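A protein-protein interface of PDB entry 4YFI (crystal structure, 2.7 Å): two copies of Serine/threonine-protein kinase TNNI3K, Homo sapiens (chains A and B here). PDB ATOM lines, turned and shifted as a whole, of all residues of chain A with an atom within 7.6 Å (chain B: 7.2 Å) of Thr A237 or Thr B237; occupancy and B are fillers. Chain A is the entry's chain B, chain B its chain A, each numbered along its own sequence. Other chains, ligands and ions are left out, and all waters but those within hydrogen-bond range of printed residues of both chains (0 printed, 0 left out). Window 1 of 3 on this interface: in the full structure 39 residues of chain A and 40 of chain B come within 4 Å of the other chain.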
ATOM      1  N   MET A 231       8.011   1.516   3.003  1.00  0.00           N
ATOM      2  CA  MET A 231       6.675   1.282   2.441  1.00  0.00           C
ATOM      3  C   MET A 231       6.221   2.391   1.523  1.00  0.00           C
ATOM      4  O   MET A 231       6.350   3.574   1.871  1.00  0.00           O
ATOM      5  CB  MET A 231       5.617   1.288   3.546  1.00  0.00           C
ATOM      6  CG  MET A 231       5.085  -0.049   3.977  1.00  0.00           C
ATOM      7  SD  MET A 231       3.446   0.195   4.687  1.00  0.00           S
ATOM      8  CE  MET A 231       3.191  -1.464   5.321  1.00  0.00           C
ATOM      9  N   ALA A 232       5.595   2.013   0.412  1.00  0.00           N
ATOM     10  CA  ALA A 232       4.909   2.983  -0.434  1.00  0.00           C
ATOM     11  C   ALA A 232       3.744   3.627   0.337  1.00  0.00           C
ATOM     12  O   ALA A 232       3.034   2.947   1.068  1.00  0.00           O
ATOM     13  CB  ALA A 232       4.406   2.323  -1.706  1.00  0.00           C
ATOM     14  N   PRO A 233       3.543   4.939   0.169  1.00  0.00           N
ATOM     15  CA  PRO A 233       2.467   5.677   0.832  1.00  0.00           C
ATOM     16  C   PRO A 233       1.086   5.053   0.689  1.00  0.00           C
ATOM     17  O   PRO A 233       0.313   5.097   1.620  1.00  0.00           O
ATOM     18  CB  PRO A 233       2.465   7.025   0.106  1.00  0.00           C
ATOM     19  CG  PRO A 233       3.833   7.177  -0.430  1.00  0.00           C
ATOM     20  CD  PRO A 233       4.308   5.791  -0.750  1.00  0.00           C
ATOM     21  N   GLU A 234       0.772   4.508  -0.479  1.00  0.00           N
ATOM     22  CA  GLU A 234      -0.543   3.906  -0.696  1.00  0.00           C
ATOM     23  C   GLU A 234      -0.681   2.600   0.066  1.00  0.00           C
ATOM     24  O   GLU A 234      -1.792   2.181   0.399  1.00  0.00           O
ATOM     25  CB  GLU A 234      -0.885   3.713  -2.194  1.00  0.00           C
ATOM     26  CG  GLU A 234      -0.090   2.649  -2.942  1.00  0.00           C
ATOM     27  CD  GLU A 234       1.195   3.165  -3.566  1.00  0.00           C
ATOM     28  OE1 GLU A 234       1.702   4.223  -3.131  1.00  0.00           O
ATOM     29  OE2 GLU A 234       1.705   2.489  -4.486  1.00  0.00           O
ATOM     30  N   VAL A 235       0.446   1.959   0.347  1.00  0.00           N
ATOM     31  CA  VAL A 235       0.428   0.765   1.164  1.00  0.00           C
ATOM     32  C   VAL A 235       0.309   1.133   2.642  1.00  0.00           C
ATOM     33  O   VAL A 235      -0.494   0.537   3.352  1.00  0.00           O
ATOM     34  CB  VAL A 235       1.651  -0.111   0.901  1.00  0.00           C
ATOM     35  CG1 VAL A 235       1.604  -1.362   1.764  1.00  0.00           C
ATOM     36  CG2 VAL A 235       1.694  -0.468  -0.579  1.00  0.00           C
ATOM     37  N   PHE A 236       1.084   2.123   3.091  1.00  0.00           N
ATOM     38  CA  PHE A 236       1.029   2.589   4.485  1.00  0.00           C
ATOM     39  C   PHE A 236      -0.391   2.935   4.877  1.00  0.00           C
ATOM     40  O   PHE A 236      -0.886   2.508   5.918  1.00  0.00           O
ATOM     41  CB  PHE A 236       1.917   3.818   4.693  1.00  0.00           C
ATOM     42  CG  PHE A 236       1.866   4.374   6.096  1.00  0.00           C
ATOM     43  CD1 PHE A 236       2.383   3.644   7.171  1.00  0.00           C
ATOM     44  CD2 PHE A 236       1.300   5.618   6.350  1.00  0.00           C
ATOM     45  CE1 PHE A 236       2.340   4.143   8.462  1.00  0.00           C
ATOM     46  CE2 PHE A 236       1.260   6.125   7.644  1.00  0.00           C
ATOM     47  CZ  PHE A 236       1.779   5.387   8.699  1.00  0.00           C
ATOM     48  N   THR A 237      -1.024   3.720   4.021  1.00  0.00           N
ATOM     49  CA  THR A 237      -2.416   4.121   4.162  1.00  0.00           C
ATOM     50  C   THR A 237      -3.392   2.953   4.330  1.00  0.00           C
ATOM     51  O   THR A 237      -4.387   3.091   5.026  1.00  0.00           O
ATOM     52  CB  THR A 237      -2.817   4.994   2.952  1.00  0.00           C
ATOM     53  OG1 THR A 237      -2.328   6.329   3.166  1.00  0.00           O
ATOM     54  CG2 THR A 237      -4.301   5.040   2.762  1.00  0.00           C
ATOM     55  N   GLN A 238      -3.119   1.814   3.705  1.00  0.00           N
ATOM     56  CA  GLN A 238      -4.024   0.665   3.800  1.00  0.00           C
ATOM     57  C   GLN A 238      -3.901  -0.111   5.105  1.00  0.00           C
ATOM     58  O   GLN A 238      -4.880  -0.682   5.579  1.00  0.00           O
ATOM     59  CB  GLN A 238      -3.829  -0.270   2.619  1.00  0.00           C
ATOM     60  CG  GLN A 238      -4.464   0.261   1.354  1.00  0.00           C
ATOM     61  CD  GLN A 238      -4.117  -0.579   0.149  1.00  0.00           C
ATOM     62  OE1 GLN A 238      -3.541  -0.080  -0.814  1.00  0.00           O
ATOM     63  NE2 GLN A 238      -4.455  -1.868   0.197  1.00  0.00           N
ATOM     64  N   CYS A 239      -2.701  -0.129   5.675  1.00  0.00           N
ATOM     65  CA  CYS A 239      -2.456  -0.756   6.969  1.00  0.00           C
ATOM     66  C   CYS A 239      -2.785   0.194   8.130  1.00  0.00           C
ATOM     67  O   CYS A 239      -2.675  -0.178   9.289  1.00  0.00           O
ATOM     68  CB  CYS A 239      -0.995  -1.212   7.049  1.00  0.00           C
ATOM     69  SG  CYS A 239      -0.509  -2.328   5.707  1.00  0.00           S
ATOM     70  N   THR A 240      -3.176   1.429   7.811  1.00  0.00           N
ATOM     71  CA  THR A 240      -3.558   2.416   8.820  1.00  0.00           C
ATOM     72  C   THR A 240      -5.076   2.460   8.981  1.00  0.00           C
ATOM     73  O   THR A 240      -5.823   2.286   8.019  1.00  0.00           O
ATOM     74  CB  THR A 240      -3.037   3.825   8.460  1.00  0.00           C
ATOM     75  OG1 THR A 240      -1.606   3.803   8.396  1.00  0.00           O
ATOM     76  CG2 THR A 240      -3.450   4.865   9.503  1.00  0.00           C
ATOM     77  N   ARG A 241      -5.511   2.702  10.215  1.00  0.00           N
ATOM     78  CA  ARG A 241      -6.926   2.754  10.567  1.00  0.00           C
ATOM     79  C   ARG A 241      -7.595   3.997   9.966  1.00  0.00           C
ATOM     80  O   ARG A 241      -7.005   5.081  10.000  1.00  0.00           O
ATOM     81  CB  ARG A 241      -7.071   2.764  12.098  1.00  0.00           C
ATOM     82  N   TYR A 242      -8.810   3.842   9.418  1.00  0.00           N
ATOM     83  CA  TYR A 242      -9.634   4.994   8.939  1.00  0.00           C
ATOM     84  C   TYR A 242     -10.181   5.860  10.107  1.00  0.00           C
ATOM     85  O   TYR A 242     -10.837   5.336  11.005  1.00  0.00           O
ATOM     86  CB  TYR A 242     -10.799   4.521   8.044  1.00  0.00           C
ATOM     87  N   ASP A 274      -9.912  12.904  -7.557  1.00  0.00           N
ATOM     88  CA  ASP A 274      -9.360  12.322  -6.333  1.00  0.00           C
ATOM     89  C   ASP A 274      -7.855  12.188  -6.420  1.00  0.00           C
ATOM     90  O   ASP A 274      -7.143  12.430  -5.437  1.00  0.00           O
ATOM     91  CB  ASP A 274      -9.971  10.954  -6.052  1.00  0.00           C
ATOM     92  N   ALA A 278      -5.024  13.747  -4.085  1.00  0.00           N
ATOM     93  CA  ALA A 278      -4.159  12.860  -3.307  1.00  0.00           C
ATOM     94  C   ALA A 278      -2.681  12.949  -3.667  1.00  0.00           C
ATOM     95  O   ALA A 278      -1.815  12.890  -2.801  1.00  0.00           O
ATOM     96  CB  ALA A 278      -4.630  11.426  -3.466  1.00  0.00           C
ATOM     97  N   TYR A 279      -2.400  13.045  -4.954  1.00  0.00           N
ATOM     98  CA  TYR A 279      -1.054  12.833  -5.464  1.00  0.00           C
ATOM     99  C   TYR A 279      -0.361  14.135  -5.793  1.00  0.00           C
ATOM    100  O   TYR A 279       0.808  14.303  -5.494  1.00  0.00           O
ATOM    101  CB  TYR A 279      -1.109  11.974  -6.727  1.00  0.00           C
ATOM    102  CG  TYR A 279      -1.666  10.572  -6.541  1.00  0.00           C
ATOM    103  CD1 TYR A 279      -1.350   9.799  -5.420  1.00  0.00           C
ATOM    104  CD2 TYR A 279      -2.470  10.000  -7.519  1.00  0.00           C
ATOM    105  CE1 TYR A 279      -1.842   8.515  -5.277  1.00  0.00           C
ATOM    106  CE2 TYR A 279      -2.963   8.715  -7.380  1.00  0.00           C
ATOM    107  CZ  TYR A 279      -2.644   7.983  -6.265  1.00  0.00           C
ATOM    108  OH  TYR A 279      -3.142   6.718  -6.148  1.00  0.00           O
ATOM    109  N   MET B 231     -13.788  12.315  -1.324  1.00  0.00           N
ATOM    110  CA  MET B 231     -12.973  11.498  -0.409  1.00  0.00           C
ATOM    111  C   MET B 231     -11.711  12.171   0.095  1.00  0.00           C
ATOM    112  O   MET B 231     -11.085  12.959  -0.608  1.00  0.00           O
ATOM    113  CB  MET B 231     -12.500  10.227  -1.094  1.00  0.00           C
ATOM    114  CG  MET B 231     -13.548   9.163  -1.240  1.00  0.00           C
ATOM    115  SD  MET B 231     -12.813   7.590  -1.694  1.00  0.00           S
ATOM    116  CE  MET B 231     -14.287   6.561  -1.579  1.00  0.00           C
ATOM    117  N   ALA B 232     -11.311  11.786   1.298  1.00  0.00           N
ATOM    118  CA  ALA B 232     -10.017  12.157   1.847  1.00  0.00           C
ATOM    119  C   ALA B 232      -8.941  11.352   1.140  1.00  0.00           C
ATOM    120  O   ALA B 232      -9.140  10.165   0.898  1.00  0.00           O
ATOM    121  CB  ALA B 232      -9.970  11.870   3.336  1.00  0.00           C
ATOM    122  N   PRO B 233      -7.796  11.985   0.820  1.00  0.00           N
ATOM    123  CA  PRO B 233      -6.706  11.297   0.130  1.00  0.00           C
ATOM    124  C   PRO B 233      -6.289   9.973   0.768  1.00  0.00           C
ATOM    125  O   PRO B 233      -6.045   9.011   0.062  1.00  0.00           O
ATOM    126  CB  PRO B 233      -5.570  12.310   0.190  1.00  0.00           C
ATOM    127  CG  PRO B 233      -6.266  13.636   0.174  1.00  0.00           C
ATOM    128  CD  PRO B 233      -7.492  13.417   1.021  1.00  0.00           C
ATOM    129  N   GLU B 234      -6.232   9.908   2.090  1.00  0.00           N
ATOM    130  CA  GLU B 234      -5.934   8.640   2.767  1.00  0.00           C
ATOM    131  C   GLU B 234      -7.067   7.599   2.724  1.00  0.00           C
ATOM    132  O   GLU B 234      -6.916   6.508   3.258  1.00  0.00           O
ATOM    133  CB  GLU B 234      -5.541   8.881   4.227  1.00  0.00           C
ATOM    134  CG  GLU B 234      -6.690   9.197   5.182  1.00  0.00           C
ATOM    135  CD  GLU B 234      -7.005  10.681   5.268  1.00  0.00           C
ATOM    136  OE1 GLU B 234      -6.578  11.471   4.384  1.00  0.00           O
ATOM    137  OE2 GLU B 234      -7.692  11.055   6.238  1.00  0.00           O
ATOM    138  N   VAL B 235      -8.207   7.944   2.141  1.00  0.00           N
ATOM    139  CA  VAL B 235      -9.280   6.979   1.917  1.00  0.00           C
ATOM    140  C   VAL B 235      -9.292   6.573   0.445  1.00  0.00           C
ATOM    141  O   VAL B 235      -9.398   5.395   0.128  1.00  0.00           O
ATOM    142  CB  VAL B 235     -10.667   7.534   2.329  1.00  0.00           C
ATOM    143  CG1 VAL B 235     -11.762   6.499   2.084  1.00  0.00           C
ATOM    144  CG2 VAL B 235     -10.672   7.971   3.795  1.00  0.00           C
ATOM    145  N   PHE B 236      -9.189   7.547  -0.450  1.00  0.00           N
ATOM    146  CA  PHE B 236      -9.029   7.261  -1.875  1.00  0.00           C
ATOM    147  C   PHE B 236      -7.941   6.200  -2.123  1.00  0.00           C
ATOM    148  O   PHE B 236      -8.036   5.357  -3.027  1.00  0.00           O
ATOM    149  CB  PHE B 236      -8.675   8.552  -2.625  1.00  0.00           C
ATOM    150  CG  PHE B 236      -8.274   8.331  -4.055  1.00  0.00           C
ATOM    151  CD1 PHE B 236      -9.211   7.921  -4.993  1.00  0.00           C
ATOM    152  CD2 PHE B 236      -6.958   8.517  -4.463  1.00  0.00           C
ATOM    153  CE1 PHE B 236      -8.847   7.707  -6.312  1.00  0.00           C
ATOM    154  CE2 PHE B 236      -6.588   8.302  -5.782  1.00  0.00           C
ATOM    155  CZ  PHE B 236      -7.534   7.900  -6.706  1.00  0.00           C
ATOM    156  N   THR B 237      -6.900   6.260  -1.313  1.00  0.00           N
ATOM    157  CA  THR B 237      -5.765   5.384  -1.447  1.00  0.00           C
ATOM    158  C   THR B 237      -6.060   4.007  -0.856  1.00  0.00           C
ATOM    159  O   THR B 237      -5.480   3.020  -1.283  1.00  0.00           O
ATOM    160  CB  THR B 237      -4.568   6.061  -0.782  1.00  0.00           C
ATOM    161  OG1 THR B 237      -4.195   7.207  -1.557  1.00  0.00           O
ATOM    162  CG2 THR B 237      -3.420   5.150  -0.688  1.00  0.00           C
ATOM    163  N   GLN B 238      -6.969   3.942   0.115  1.00  0.00           N
ATOM    164  CA  GLN B 238      -7.501   2.655   0.609  1.00  0.00           C
ATOM    165  C   GLN B 238      -8.417   1.906  -0.377  1.00  0.00           C
ATOM    166  O   GLN B 238      -8.845   0.789  -0.089  1.00  0.00           O
ATOM    167  CB  GLN B 238      -8.259   2.842   1.933  1.00  0.00           C
ATOM    168  CG  GLN B 238      -7.448   2.464   3.160  1.00  0.00           C
ATOM    169  CD  GLN B 238      -8.300   2.145   4.378  1.00  0.00           C
ATOM    170  OE1 GLN B 238      -9.512   2.386   4.397  1.00  0.00           O
ATOM    171  NE2 GLN B 238      -7.662   1.598   5.413  1.00  0.00           N
ATOM    172  N   CYS B 239      -8.725   2.520  -1.519  1.00  0.00           N
ATOM    173  CA  CYS B 239      -9.566   1.901  -2.549  1.00  0.00           C
ATOM    174  C   CYS B 239      -8.775   1.148  -3.620  1.00  0.00           C
ATOM    175  O   CYS B 239      -9.329   0.290  -4.306  1.00  0.00           O
ATOM    176  CB  CYS B 239     -10.457   2.958  -3.200  1.00  0.00           C
ATOM    177  SG  CYS B 239     -11.634   3.681  -2.035  1.00  0.00           S
ATOM    178  N   THR B 240      -7.491   1.468  -3.766  1.00  0.00           N
ATOM    179  CA  THR B 240      -6.599   0.743  -4.679  1.00  0.00           C
ATOM    180  C   THR B 240      -5.806  -0.315  -3.900  1.00  0.00           C
ATOM    181  O   THR B 240      -5.486  -0.113  -2.730  1.00  0.00           O
ATOM    182  CB  THR B 240      -5.623   1.717  -5.366  1.00  0.00           C
ATOM    183  OG1 THR B 240      -6.323   2.922  -5.715  1.00  0.00           O
ATOM    184  CG2 THR B 240      -5.004   1.086  -6.622  1.00  0.00           C
ATOM    185  N   ARG B 241      -5.503  -1.442  -4.541  1.00  0.00           N
ATOM    186  CA  ARG B 241      -4.736  -2.515  -3.886  1.00  0.00           C
ATOM    187  C   ARG B 241      -3.225  -2.351  -4.130  1.00  0.00           C
ATOM    188  O   ARG B 241      -2.806  -1.491  -4.925  1.00  0.00           O
ATOM    189  CB  ARG B 241      -5.214  -3.882  -4.368  1.00  0.00           C
ATOM    190  N   ALA B 278       3.888   9.917   3.476  1.00  0.00           N
ATOM    191  CA  ALA B 278       2.516   9.773   2.982  1.00  0.00           C
ATOM    192  C   ALA B 278       1.710  11.073   3.104  1.00  0.00           C
ATOM    193  O   ALA B 278       1.164  11.577   2.129  1.00  0.00           O
ATOM    194  CB  ALA B 278       1.815   8.641   3.723  1.00  0.00           C
ATOM    195  N   TYR B 279       1.655  11.622   4.307  1.00  0.00           N
ATOM    196  CA  TYR B 279       0.808  12.771   4.582  1.00  0.00           C
ATOM    197  C   TYR B 279       1.451  14.123   4.244  1.00  0.00           C
ATOM    198  O   TYR B 279       0.767  15.047   3.792  1.00  0.00           O
ATOM    199  CB  TYR B 279       0.412  12.768   6.048  1.00  0.00           C
ATOM    200  CG  TYR B 279      -0.227  11.487   6.515  1.00  0.00           C
ATOM    201  CD1 TYR B 279      -1.219  10.865   5.767  1.00  0.00           C
ATOM    202  CD2 TYR B 279       0.141  10.919   7.724  1.00  0.00           C
ATOM    203  CE1 TYR B 279      -1.815   9.703   6.213  1.00  0.00           C
ATOM    204  CE2 TYR B 279      -0.443   9.760   8.167  1.00  0.00           C
ATOM    205  CZ  TYR B 279      -1.422   9.160   7.411  1.00  0.00           C
ATOM    206  OH  TYR B 279      -1.987   7.993   7.861  1.00  0.00           O
ATOM    207  N   ALA B 304       4.522  10.088  -5.597  1.00  0.00           N
ATOM    208  CA  ALA B 304       3.354   9.734  -4.791  1.00  0.00           C
ATOM    209  C   ALA B 304       2.299   9.117  -5.686  1.00  0.00           C
ATOM    210  O   ALA B 304       1.536   8.249  -5.244  1.00  0.00           O
ATOM    211  CB  ALA B 304       2.795  10.945  -4.063  1.00  0.00           C
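Pro A233 touches Ala B278 (CB to CA, 3.98 Å).
Glu A234 touches Thr B237.
CE2 of Phe A236 touches OH of Tyr B279 (3.8 Å).
Thr B237 touches Thr A237 (CG2 to CG2, 3.6 Å).
Thr A237 touches Gln B238.
OE1 of Gln A238 touches O of Thr B237 (3.7 Å).
Tyr B279 touches Thr A240.
Phe B236 touches Asp A274 (CD1 to CB, 3.3 Å).
Tyr A279 touches Phe B236.
Ala B304 touches Tyr A279.
Of the 15 printed residues of chain A, 9 touch a printed residue of chain B.
Hydrophobic or aromatic side chains of chain A that line the printed part of chain B: Pro A233, Phe A236, Ala A278 and Tyr A279.
Hydrophobic or aromatic side chains of chain B that line the printed part of chain A: Pro B233, Phe B236 and Tyr B279.
Among the printed residues, no Asp or Glu carboxylate lies within 4 Å of a Lys or Arg side-chain nitrogen of the other chain.
Of chain B, only Glu B234 (3.0 Å), Thr B237 (3.6 Å) and Gln B238 (3.6 Å) come within 4 Å of Thr A237.
Tyr A242 touches none of the printed residues of chain B.
Printed residues of chain A within 4 Å of Glu B234: Thr A237 (3.0 Å).
Val B235 touches none of the printed residues of chain A.
Of chain A, only Glu A234 (3.1 Å), Thr A237 (3.6 Å) and Gln A238 (3.7 Å) come within 4 Å of Thr B237.
Of the printed residues of chain A, Ala B304 touches Tyr A279.
The nearest residue of chain B that does not touch Thr A237 is Tyr B279 (4.6 Å).
Phe A236 touches Tyr B279, and with the chains exchanged Tyr A279 touches Phe B236.
Gln A238 touches its own counterpart, Gln B238.
Thr A240 touches Tyr B279, but with the chains exchanged Tyr A279 does not touch Thr B240 (5.0 Å).
Ala A278 touches Phe B236, but with the chains exchanged Phe A236 does not touch Ala B278 (4.04 Å).
Of the 16 pairs that touch across the chains among the printed residues, 12 have their exchanged pair printed and touching as well.
The side-chain amide oxygen (OE1) of Gln A238 lies close to the backbone carbonyl oxygen (O) of Thr B240, 2.7 Å away.
The side-chain amide nitrogen (NE2) of Gln B238 sits at hydrogen-bond distance from the backbone carbonyl oxygen (O) of Thr A240 (3.3 Å).
The side-chain amide oxygen (OE1) of Gln A238 sits close to the backbone carbonyl oxygen (O) of Glu A234 (3.1 Å).
O of Pro A233 sits at hydrogen-bond distance from OG1 of Thr A237 (3.3 Å).
The backbone carbonyl oxygen (O) of Phe A236 lies within hydrogen-bond range of the side-chain hydroxyl (OG1) of Thr A240 (2.9 Å).
OG1 of Thr B237 lies within hydrogen-bond range of O of Pro B233.
The side-chain sulfur (SD) of Met A231 sits close to the backbone NH (N) of Phe A236 (3.4 Å).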
